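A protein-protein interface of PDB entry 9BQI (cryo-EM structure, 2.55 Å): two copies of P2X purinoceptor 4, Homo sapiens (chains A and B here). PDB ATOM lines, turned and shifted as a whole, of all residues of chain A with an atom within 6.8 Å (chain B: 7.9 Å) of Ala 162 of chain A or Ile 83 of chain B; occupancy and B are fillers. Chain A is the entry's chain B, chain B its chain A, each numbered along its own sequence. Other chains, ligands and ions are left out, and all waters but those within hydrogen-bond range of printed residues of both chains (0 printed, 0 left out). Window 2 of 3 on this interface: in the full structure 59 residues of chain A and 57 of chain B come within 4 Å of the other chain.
The side-chain amide oxygen (OE1) of Gln 113 of chain A is in hydrogen-bond range of the backbone NH (N) of Ile 83 of chain B (3.3 Å).
O of Ile 83 of chain B sits at hydrogen-bond distance from NE1 of Trp 164 of chain A, at 3.5 Å.
NH2 of Arg 309 of chain A lies within salt-bridge range of OD2 of Asp 85 of chain B, at 2.7 Å.
OD2 of Asp 88 of chain B lies within hydrogen-bond range of NE1 of Trp 164 of chain A, at 3.2 Å.
The side-chain carboxylate (OD2) of Asp 88 of chain B lies within salt-bridge range of the guanidinium group (NH1) of Arg 309 of chain A.
O of Thr 74 of chain B lies within hydrogen-bond range of N of Arg 82 of chain B (2.9 Å).
N of Asp 85 of chain B lies within hydrogen-bond range of OD2 of Asp 88 of chain B, at 3.4 Å.
The backbone NH of Ala 163 of chain A is in hydrogen-bond range of the backbone carbonyl oxygen of Gly 114 of chain A (3.1 Å).
O of Val 144 of chain A lies within hydrogen-bond range of N of Ala 162 of chain A (2.9 Å).
The side-chain sulfur (SG) of Cys 165 of chain A is disulfide-bonded to the side-chain sulfur (SG) of Cys 116 of chain A, 2.0 Å away.
Among the printed residues, merely in contact across the chains: Val 144 of chain A with Val 73 of chain B, Ala 162 of chain A with Ile 83 of chain B, Trp 164 of chain A with Asp 85 of chain B, Gly 143 of chain A with Val 71 of chain B, Gln 113 of chain A with Arg 82 of chain B, Val 144 of chain A with Val 71 of chain B and Ala 163 of chain A with Ile 83 of chain B.
Ala 162 of chain A touches one residue of chain B.
Ile 83 of chain B touches just these residues of chain A: Gln 113 (3.3 Å), Ala 162 (3.3 Å), Ala 163 (3.9 Å) and Trp 164 (3.5 Å).
Of the printed residues of chain B, Gln 113 of chain A touches Arg 82 (3.8 Å) and Ile 83 (3.3 Å).
Of the printed residues of chain A, Asp 88 of chain B touches Trp 164 (3.2 Å) and Arg 309 (3.5 Å).
Of the printed residues of chain A, Val 73 of chain B touches Val 144 (3.3 Å).
Printed residues of chain A within 4 Å of Val 71 of chain B: Gly 143 and Val 144.
Of the printed residues of chain B, Arg 309 of chain A touches Asp 85 and Asp 88.
Cys 165 of chain A touches none of the printed residues of chain B.
Tyr 89 of chain B touches none of the printed residues of chain A.
Of the 16 printed residues of chain B, 6 touch a printed residue of chain A.
Printed residues of chain B that touch a printed residue of chain A: Val 71, Val 73, Arg 82, Ile 83, Asp 85 and Asp 88.
Hydrophobic or aromatic side chains of chain A within 4 Å of the printed part of chain B: Val 144 and Trp 164.
Along chain A the printed residues that touch a printed residue of chain B span positions 113 to 309.
Among the printed residues, 12 pairs touch across the chains.
Among the printed residues, Asp or Glu carboxylates within 4 Å of a Lys or Arg side-chain nitrogen of the other chain: Arg 309 of chain A with Asp 85 of chain B and Arg 309 of chain A with Asp 88 of chain B.
No position is printed for both chains.
Of the 12 pairs that touch across the chains among the printed residues, none has its exchanged pair printed and touching as well.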
ATOM      1  N   GLN A 113      14.828  -9.289 -24.429  1.00  0.00           N
ATOM      2  CA  GLN A 113      13.938 -10.336 -23.951  1.00  0.00           C
ATOM      3  C   GLN A 113      14.316 -11.667 -24.581  1.00  0.00           C
ATOM      4  O   GLN A 113      14.597 -11.742 -25.781  1.00  0.00           O
ATOM      5  CB  GLN A 113      12.483  -9.994 -24.279  1.00  0.00           C
ATOM      6  CG  GLN A 113      12.046  -8.595 -23.889  1.00  0.00           C
ATOM      7  CD  GLN A 113      11.382  -8.556 -22.537  1.00  0.00           C
ATOM      8  OE1 GLN A 113      11.645  -9.395 -21.679  1.00  0.00           O
ATOM      9  NE2 GLN A 113      10.510  -7.580 -22.339  1.00  0.00           N
ATOM     10  N   GLY A 114      14.323 -12.718 -23.775  1.00  0.00           N
ATOM     11  CA  GLY A 114      14.681 -14.027 -24.275  1.00  0.00           C
ATOM     12  C   GLY A 114      14.976 -14.976 -23.132  1.00  0.00           C
ATOM     13  O   GLY A 114      14.637 -14.717 -21.977  1.00  0.00           O
ATOM     14  N   LEU A 115      15.621 -16.080 -23.490  1.00  0.00           N
ATOM     15  CA  LEU A 115      15.991 -17.122 -22.546  1.00  0.00           C
ATOM     16  C   LEU A 115      17.501 -17.109 -22.353  1.00  0.00           C
ATOM     17  O   LEU A 115      18.257 -17.026 -23.325  1.00  0.00           O
ATOM     18  CB  LEU A 115      15.537 -18.491 -23.051  1.00  0.00           C
ATOM     19  CG  LEU A 115      14.027 -18.701 -23.184  1.00  0.00           C
ATOM     20  CD1 LEU A 115      13.738 -20.039 -23.837  1.00  0.00           C
ATOM     21  CD2 LEU A 115      13.339 -18.610 -21.837  1.00  0.00           C
ATOM     22  N   CYS A 116      17.936 -17.184 -21.100  1.00  0.00           N
ATOM     23  CA  CYS A 116      19.353 -17.110 -20.781  1.00  0.00           C
ATOM     24  C   CYS A 116      19.590 -17.774 -19.435  1.00  0.00           C
ATOM     25  O   CYS A 116      18.668 -17.878 -18.619  1.00  0.00           O
ATOM     26  CB  CYS A 116      19.844 -15.658 -20.757  1.00  0.00           C
ATOM     27  SG  CYS A 116      18.919 -14.583 -19.643  1.00  0.00           S
ATOM     28  N   ASN A 142      14.128 -11.690 -11.094  1.00  0.00           N
ATOM     29  CA  ASN A 142      14.523 -11.087 -12.359  1.00  0.00           C
ATOM     30  C   ASN A 142      13.996 -11.842 -13.569  1.00  0.00           C
ATOM     31  O   ASN A 142      14.004 -11.290 -14.673  1.00  0.00           O
ATOM     32  CB  ASN A 142      16.051 -11.000 -12.442  1.00  0.00           C
ATOM     33  CG  ASN A 142      16.694 -12.334 -12.748  1.00  0.00           C
ATOM     34  OD1 ASN A 142      16.276 -13.370 -12.232  1.00  0.00           O
ATOM     35  ND2 ASN A 142      17.723 -12.317 -13.585  1.00  0.00           N
ATOM     36  N   GLY A 143      13.537 -13.077 -13.391  1.00  0.00           N
ATOM     37  CA  GLY A 143      12.996 -13.853 -14.489  1.00  0.00           C
ATOM     38  C   GLY A 143      12.148 -14.990 -13.966  1.00  0.00           C
ATOM     39  O   GLY A 143      12.098 -15.254 -12.763  1.00  0.00           O
ATOM     40  N   VAL A 144      11.477 -15.664 -14.894  1.00  0.00           N
ATOM     41  CA  VAL A 144      10.629 -16.810 -14.590  1.00  0.00           C
ATOM     42  C   VAL A 144      11.311 -18.060 -15.124  1.00  0.00           C
ATOM     43  O   VAL A 144      11.610 -18.149 -16.320  1.00  0.00           O
ATOM     44  CB  VAL A 144       9.221 -16.648 -15.190  1.00  0.00           C
ATOM     45  CG1 VAL A 144       8.373 -17.874 -14.903  1.00  0.00           C
ATOM     46  CG2 VAL A 144       8.557 -15.398 -14.640  1.00  0.00           C
ATOM     47  N   SER A 145      11.554 -19.023 -14.239  1.00  0.00           N
ATOM     48  CA  SER A 145      12.270 -20.229 -14.627  1.00  0.00           C
ATOM     49  C   SER A 145      11.462 -21.035 -15.636  1.00  0.00           C
ATOM     50  O   SER A 145      10.236 -21.123 -15.548  1.00  0.00           O
ATOM     51  CB  SER A 145      12.571 -21.082 -13.395  1.00  0.00           C
ATOM     52  OG  SER A 145      13.231 -22.281 -13.759  1.00  0.00           O
ATOM     53  N   THR A 146      12.166 -21.627 -16.600  1.00  0.00           N
ATOM     54  CA  THR A 146      11.539 -22.468 -17.610  1.00  0.00           C
ATOM     55  C   THR A 146      11.645 -23.956 -17.302  1.00  0.00           C
ATOM     56  O   THR A 146      10.881 -24.744 -17.868  1.00  0.00           O
ATOM     57  CB  THR A 146      12.163 -22.206 -18.986  1.00  0.00           C
ATOM     58  OG1 THR A 146      13.551 -22.558 -18.959  1.00  0.00           O
ATOM     59  CG2 THR A 146      12.026 -20.743 -19.364  1.00  0.00           C
ATOM     60  N   GLU A 160      17.714 -22.160 -16.430  1.00  0.00           N
ATOM     61  CA  GLU A 160      17.333 -21.170 -17.425  1.00  0.00           C
ATOM     62  C   GLU A 160      16.133 -20.363 -16.945  1.00  0.00           C
ATOM     63  O   GLU A 160      15.251 -20.879 -16.254  1.00  0.00           O
ATOM     64  CB  GLU A 160      17.005 -21.852 -18.752  1.00  0.00           C
ATOM     65  CG  GLU A 160      16.983 -20.923 -19.948  1.00  0.00           C
ATOM     66  CD  GLU A 160      16.820 -21.674 -21.252  1.00  0.00           C
ATOM     67  OE1 GLU A 160      16.368 -22.836 -21.214  1.00  0.00           O
ATOM     68  OE2 GLU A 160      17.160 -21.111 -22.313  1.00  0.00           O
ATOM     69  N   VAL A 161      16.108 -19.086 -17.320  1.00  0.00           N
ATOM     70  CA  VAL A 161      14.998 -18.199 -17.000  1.00  0.00           C
ATOM     71  C   VAL A 161      14.630 -17.405 -18.243  1.00  0.00           C
ATOM     72  O   VAL A 161      15.443 -17.221 -19.151  1.00  0.00           O
ATOM     73  CB  VAL A 161      15.329 -17.238 -15.835  1.00  0.00           C
ATOM     74  CG1 VAL A 161      15.420 -17.999 -14.525  1.00  0.00           C
ATOM     75  CG2 VAL A 161      16.613 -16.474 -16.112  1.00  0.00           C
ATOM     76  N   ALA A 162      13.385 -16.935 -18.277  1.00  0.00           N
ATOM     77  CA  ALA A 162      12.920 -15.992 -19.286  1.00  0.00           C
ATOM     78  C   ALA A 162      12.947 -14.603 -18.665  1.00  0.00           C
ATOM     79  O   ALA A 162      12.172 -14.313 -17.749  1.00  0.00           O
ATOM     80  CB  ALA A 162      11.520 -16.356 -19.770  1.00  0.00           C
ATOM     81  N   ALA A 163      13.837 -13.749 -19.155  1.00  0.00           N
ATOM     82  CA  ALA A 163      14.024 -12.424 -18.582  1.00  0.00           C
ATOM     83  C   ALA A 163      14.674 -11.529 -19.629  1.00  0.00           C
ATOM     84  O   ALA A 163      14.864 -11.930 -20.782  1.00  0.00           O
ATOM     85  CB  ALA A 163      14.868 -12.504 -17.308  1.00  0.00           C
ATOM     86  N   TRP A 164      15.000 -10.305 -19.229  1.00  0.00           N
ATOM     87  CA  TRP A 164      15.914  -9.483 -20.006  1.00  0.00           C
ATOM     88  C   TRP A 164      17.312 -10.068 -19.883  1.00  0.00           C
ATOM     89  O   TRP A 164      17.783 -10.335 -18.774  1.00  0.00           O
ATOM     90  CB  TRP A 164      15.901  -8.044 -19.504  1.00  0.00           C
ATOM     91  CG  TRP A 164      14.642  -7.285 -19.771  1.00  0.00           C
ATOM     92  CD1 TRP A 164      13.546  -7.209 -18.965  1.00  0.00           C
ATOM     93  CD2 TRP A 164      14.359  -6.465 -20.910  1.00  0.00           C
ATOM     94  NE1 TRP A 164      12.596  -6.401 -19.534  1.00  0.00           N
ATOM     95  CE2 TRP A 164      13.070  -5.932 -20.729  1.00  0.00           C
ATOM     96  CE3 TRP A 164      15.070  -6.135 -22.065  1.00  0.00           C
ATOM     97  CZ2 TRP A 164      12.477  -5.085 -21.660  1.00  0.00           C
ATOM     98  CZ3 TRP A 164      14.478  -5.300 -22.990  1.00  0.00           C
ATOM     99  CH2 TRP A 164      13.196  -4.783 -22.783  1.00  0.00           C
ATOM    100  N   CYS A 165      17.976 -10.277 -21.016  1.00  0.00           N
ATOM    101  CA  CYS A 165      19.216 -11.031 -21.020  1.00  0.00           C
ATOM    102  C   CYS A 165      20.319 -10.247 -21.718  1.00  0.00           C
ATOM    103  O   CYS A 165      20.058  -9.562 -22.711  1.00  0.00           O
ATOM    104  CB  CYS A 165      19.015 -12.383 -21.717  1.00  0.00           C
ATOM    105  SG  CYS A 165      17.805 -13.446 -20.902  1.00  0.00           S
ATOM    106  N   ARG A 309      17.496  -2.503 -23.825  1.00  0.00           N
ATOM    107  CA  ARG A 309      17.508  -1.693 -22.617  1.00  0.00           C
ATOM    108  C   ARG A 309      18.860  -1.801 -21.932  1.00  0.00           C
ATOM    109  O   ARG A 309      19.566  -2.804 -22.059  1.00  0.00           O
ATOM    110  CB  ARG A 309      16.385  -2.084 -21.641  1.00  0.00           C
ATOM    111  CG  ARG A 309      16.706  -3.218 -20.679  1.00  0.00           C
ATOM    112  CD  ARG A 309      15.716  -3.257 -19.540  1.00  0.00           C
ATOM    113  NE  ARG A 309      16.086  -4.249 -18.542  1.00  0.00           N
ATOM    114  CZ  ARG A 309      15.360  -4.548 -17.475  1.00  0.00           C
ATOM    115  NH1 ARG A 309      14.220  -3.930 -17.221  1.00  0.00           N
ATOM    116  NH2 ARG A 309      15.785  -5.494 -16.645  1.00  0.00           N
ATOM    117  N   GLY B  70       9.045  -8.823  -7.610  1.00  0.00           N
ATOM    118  CA  GLY B  70       8.138  -9.632  -8.402  1.00  0.00           C
ATOM    119  C   GLY B  70       8.393  -9.430  -9.881  1.00  0.00           C
ATOM    120  O   GLY B  70       8.795  -8.358 -10.331  1.00  0.00           O
ATOM    121  N   VAL B  71       8.156 -10.482 -10.656  1.00  0.00           N
ATOM    122  CA  VAL B  71       8.333 -10.458 -12.103  1.00  0.00           C
ATOM    123  C   VAL B  71       7.096 -11.068 -12.746  1.00  0.00           C
ATOM    124  O   VAL B  71       6.617 -12.122 -12.318  1.00  0.00           O
ATOM    125  CB  VAL B  71       9.617 -11.208 -12.524  1.00  0.00           C
ATOM    126  CG1 VAL B  71       9.554 -12.667 -12.104  1.00  0.00           C
ATOM    127  CG2 VAL B  71       9.850 -11.080 -14.021  1.00  0.00           C
ATOM    128  N   ALA B  72       6.576 -10.398 -13.773  1.00  0.00           N
ATOM    129  CA  ALA B  72       5.356 -10.808 -14.454  1.00  0.00           C
ATOM    130  C   ALA B  72       5.654 -11.168 -15.903  1.00  0.00           C
ATOM    131  O   ALA B  72       6.583 -10.635 -16.516  1.00  0.00           O
ATOM    132  CB  ALA B  72       4.296  -9.703 -14.408  1.00  0.00           C
ATOM    133  N   VAL B  73       4.847 -12.075 -16.448  1.00  0.00           N
ATOM    134  CA  VAL B  73       5.004 -12.570 -17.811  1.00  0.00           C
ATOM    135  C   VAL B  73       3.688 -12.363 -18.546  1.00  0.00           C
ATOM    136  O   VAL B  73       2.624 -12.726 -18.034  1.00  0.00           O
ATOM    137  CB  VAL B  73       5.401 -14.058 -17.831  1.00  0.00           C
ATOM    138  CG1 VAL B  73       5.459 -14.580 -19.257  1.00  0.00           C
ATOM    139  CG2 VAL B  73       6.718 -14.268 -17.112  1.00  0.00           C
ATOM    140  N   THR B  74       3.757 -11.778 -19.741  1.00  0.00           N
ATOM    141  CA  THR B  74       2.588 -11.592 -20.588  1.00  0.00           C
ATOM    142  C   THR B  74       2.928 -11.978 -22.019  1.00  0.00           C
ATOM    143  O   THR B  74       4.051 -11.757 -22.480  1.00  0.00           O
ATOM    144  CB  THR B  74       2.082 -10.140 -20.555  1.00  0.00           C
ATOM    145  OG1 THR B  74       2.868  -9.334 -21.438  1.00  0.00           O
ATOM    146  CG2 THR B  74       2.152  -9.572 -19.146  1.00  0.00           C
ATOM    147  N   ASN B  75       1.952 -12.562 -22.715  1.00  0.00           N
ATOM    148  CA  ASN B  75       2.068 -12.903 -24.134  1.00  0.00           C
ATOM    149  C   ASN B  75       0.778 -12.449 -24.809  1.00  0.00           C
ATOM    150  O   ASN B  75      -0.186 -13.215 -24.904  1.00  0.00           O
ATOM    151  CB  ASN B  75       2.317 -14.398 -24.337  1.00  0.00           C
ATOM    152  CG  ASN B  75       2.675 -14.739 -25.775  1.00  0.00           C
ATOM    153  OD1 ASN B  75       2.350 -13.990 -26.694  1.00  0.00           O
ATOM    154  ND2 ASN B  75       3.346 -15.870 -25.975  1.00  0.00           N
ATOM    155  N   GLY B  80       3.344  -8.770 -27.782  1.00  0.00           N
ATOM    156  CA  GLY B  80       4.113  -9.997 -27.809  1.00  0.00           C
ATOM    157  C   GLY B  80       4.581 -10.447 -26.436  1.00  0.00           C
ATOM    158  O   GLY B  80       4.277  -9.847 -25.401  1.00  0.00           O
ATOM    159  N   PHE B  81       5.344 -11.539 -26.443  1.00  0.00           N
ATOM    160  CA  PHE B  81       5.931 -12.050 -25.211  1.00  0.00           C
ATOM    161  C   PHE B  81       6.828 -11.001 -24.573  1.00  0.00           C
ATOM    162  O   PHE B  81       7.650 -10.370 -25.242  1.00  0.00           O
ATOM    163  CB  PHE B  81       6.736 -13.319 -25.488  1.00  0.00           C
ATOM    164  CG  PHE B  81       6.842 -14.241 -24.304  1.00  0.00           C
ATOM    165  CD1 PHE B  81       5.772 -15.025 -23.919  1.00  0.00           C
ATOM    166  CD2 PHE B  81       8.014 -14.313 -23.572  1.00  0.00           C
ATOM    167  CE1 PHE B  81       5.869 -15.869 -22.830  1.00  0.00           C
ATOM    168  CE2 PHE B  81       8.117 -15.157 -22.483  1.00  0.00           C
ATOM    169  CZ  PHE B  81       7.042 -15.934 -22.112  1.00  0.00           C
ATOM    170  N   ARG B  82       6.667 -10.820 -23.264  1.00  0.00           N
ATOM    171  CA  ARG B  82       7.448  -9.834 -22.539  1.00  0.00           C
ATOM    172  C   ARG B  82       7.610 -10.261 -21.092  1.00  0.00           C
ATOM    173  O   ARG B  82       6.878 -11.108 -20.579  1.00  0.00           O
ATOM    174  CB  ARG B  82       6.811  -8.447 -22.600  1.00  0.00           C
ATOM    175  CG  ARG B  82       6.799  -7.847 -23.982  1.00  0.00           C
ATOM    176  CD  ARG B  82       6.118  -6.511 -23.983  1.00  0.00           C
ATOM    177  NE  ARG B  82       6.858  -5.546 -23.180  1.00  0.00           N
ATOM    178  CZ  ARG B  82       7.845  -4.786 -23.638  1.00  0.00           C
ATOM    179  NH1 ARG B  82       8.249  -4.861 -24.895  1.00  0.00           N
ATOM    180  NH2 ARG B  82       8.443  -3.935 -22.811  1.00  0.00           N
ATOM    181  N   ILE B  83       8.589  -9.642 -20.443  1.00  0.00           N
ATOM    182  CA  ILE B  83       8.895  -9.850 -19.036  1.00  0.00           C
ATOM    183  C   ILE B  83       8.871  -8.485 -18.374  1.00  0.00           C
ATOM    184  O   ILE B  83       9.376  -7.508 -18.936  1.00  0.00           O
ATOM    185  CB  ILE B  83      10.266 -10.532 -18.838  1.00  0.00           C
ATOM    186  CG1 ILE B  83      10.316 -11.876 -19.573  1.00  0.00           C
ATOM    187  CG2 ILE B  83      10.566 -10.716 -17.360  1.00  0.00           C
ATOM    188  CD1 ILE B  83       9.424 -12.938 -18.989  1.00  0.00           C
ATOM    189  N   TRP B  84       8.259  -8.409 -17.200  1.00  0.00           N
ATOM    190  CA  TRP B  84       8.122  -7.156 -16.465  1.00  0.00           C
ATOM    191  C   TRP B  84       8.790  -7.325 -15.108  1.00  0.00           C
ATOM    192  O   TRP B  84       8.233  -7.956 -14.205  1.00  0.00           O
ATOM    193  CB  TRP B  84       6.653  -6.761 -16.330  1.00  0.00           C
ATOM    194  CG  TRP B  84       5.942  -6.746 -17.643  1.00  0.00           C
ATOM    195  CD1 TRP B  84       5.383  -7.808 -18.287  1.00  0.00           C
ATOM    196  CD2 TRP B  84       5.730  -5.609 -18.483  1.00  0.00           C
ATOM    197  NE1 TRP B  84       4.834  -7.404 -19.477  1.00  0.00           N
ATOM    198  CE2 TRP B  84       5.032  -6.057 -19.621  1.00  0.00           C
ATOM    199  CE3 TRP B  84       6.060  -4.255 -18.384  1.00  0.00           C
ATOM    200  CZ2 TRP B  84       4.661  -5.200 -20.650  1.00  0.00           C
ATOM    201  CZ3 TRP B  84       5.688  -3.407 -19.404  1.00  0.00           C
ATOM    202  CH2 TRP B  84       4.994  -3.880 -20.523  1.00  0.00           C
ATOM    203  N   ASP B  85       9.987  -6.765 -14.973  1.00  0.00           N
ATOM    204  CA  ASP B  85      10.699  -6.716 -13.711  1.00  0.00           C
ATOM    205  C   ASP B  85      10.503  -5.341 -13.079  1.00  0.00           C
ATOM    206  O   ASP B  85       9.816  -4.472 -13.618  1.00  0.00           O
ATOM    207  CB  ASP B  85      12.178  -7.044 -13.914  1.00  0.00           C
ATOM    208  CG  ASP B  85      12.863  -6.087 -14.862  1.00  0.00           C
ATOM    209  OD1 ASP B  85      12.262  -5.750 -15.901  1.00  0.00           O
ATOM    210  OD2 ASP B  85      14.002  -5.671 -14.572  1.00  0.00           O
ATOM    211  N   VAL B  86      11.119  -5.141 -11.914  1.00  0.00           N
ATOM    212  CA  VAL B  86      10.844  -3.938 -11.136  1.00  0.00           C
ATOM    213  C   VAL B  86      11.188  -2.685 -11.926  1.00  0.00           C
ATOM    214  O   VAL B  86      10.530  -1.650 -11.778  1.00  0.00           O
ATOM    215  CB  VAL B  86      11.599  -3.993  -9.795  1.00  0.00           C
ATOM    216  CG1 VAL B  86      13.088  -3.738 -10.000  1.00  0.00           C
ATOM    217  CG2 VAL B  86      11.003  -2.999  -8.814  1.00  0.00           C
ATOM    218  N   ASP B  88      10.592  -2.033 -14.879  1.00  0.00           N
ATOM    219  CA  ASP B  88       9.586  -1.763 -15.900  1.00  0.00           C
ATOM    220  C   ASP B  88       8.286  -1.209 -15.329  1.00  0.00           C
ATOM    221  O   ASP B  88       7.800  -0.177 -15.798  1.00  0.00           O
ATOM    222  CB  ASP B  88       9.278  -3.035 -16.695  1.00  0.00           C
ATOM    223  CG  ASP B  88      10.412  -3.449 -17.601  1.00  0.00           C
ATOM    224  OD1 ASP B  88      10.890  -2.606 -18.384  1.00  0.00           O
ATOM    225  OD2 ASP B  88      10.809  -4.628 -17.550  1.00  0.00           O
ATOM    226  N   TYR B  89       7.705  -1.873 -14.332  1.00  0.00           N
ATOM    227  CA  TYR B  89       6.347  -1.566 -13.897  1.00  0.00           C
ATOM    228  C   TYR B  89       6.281  -0.557 -12.756  1.00  0.00           C
ATOM    229  O   TYR B  89       5.177  -0.188 -12.348  1.00  0.00           O
ATOM    230  CB  TYR B  89       5.612  -2.855 -13.498  1.00  0.00           C
ATOM    231  CG  TYR B  89       6.297  -3.704 -12.448  1.00  0.00           C
ATOM    232  CD1 TYR B  89       6.425  -3.262 -11.139  1.00  0.00           C
ATOM    233  CD2 TYR B  89       6.795  -4.958 -12.762  1.00  0.00           C
ATOM    234  CE1 TYR B  89       7.039  -4.033 -10.184  1.00  0.00           C
ATOM    235  CE2 TYR B  89       7.409  -5.737 -11.810  1.00  0.00           C
ATOM    236  CZ  TYR B  89       7.527  -5.271 -10.521  1.00  0.00           C
ATOM    237  OH  TYR B  89       8.142  -6.037  -9.564  1.00  0.00           O
ATOM    238  N   LEU B 179      -1.216  -6.250 -16.344  1.00  0.00           N
ATOM    239  CA  LEU B 179      -0.392  -6.853 -15.295  1.00  0.00           C
ATOM    240  C   LEU B 179      -1.297  -7.233 -14.128  1.00  0.00           C
ATOM    241  O   LEU B 179      -1.325  -6.585 -13.084  1.00  0.00           O
ATOM    242  CB  LEU B 179       0.719  -5.909 -14.845  1.00  0.00           C
ATOM    243  CG  LEU B 179       2.044  -5.932 -15.605  1.00  0.00           C
ATOM    244  CD1 LEU B 179       1.923  -5.253 -16.947  1.00  0.00           C
ATOM    245  CD2 LEU B 179       3.129  -5.284 -14.763  1.00  0.00           C
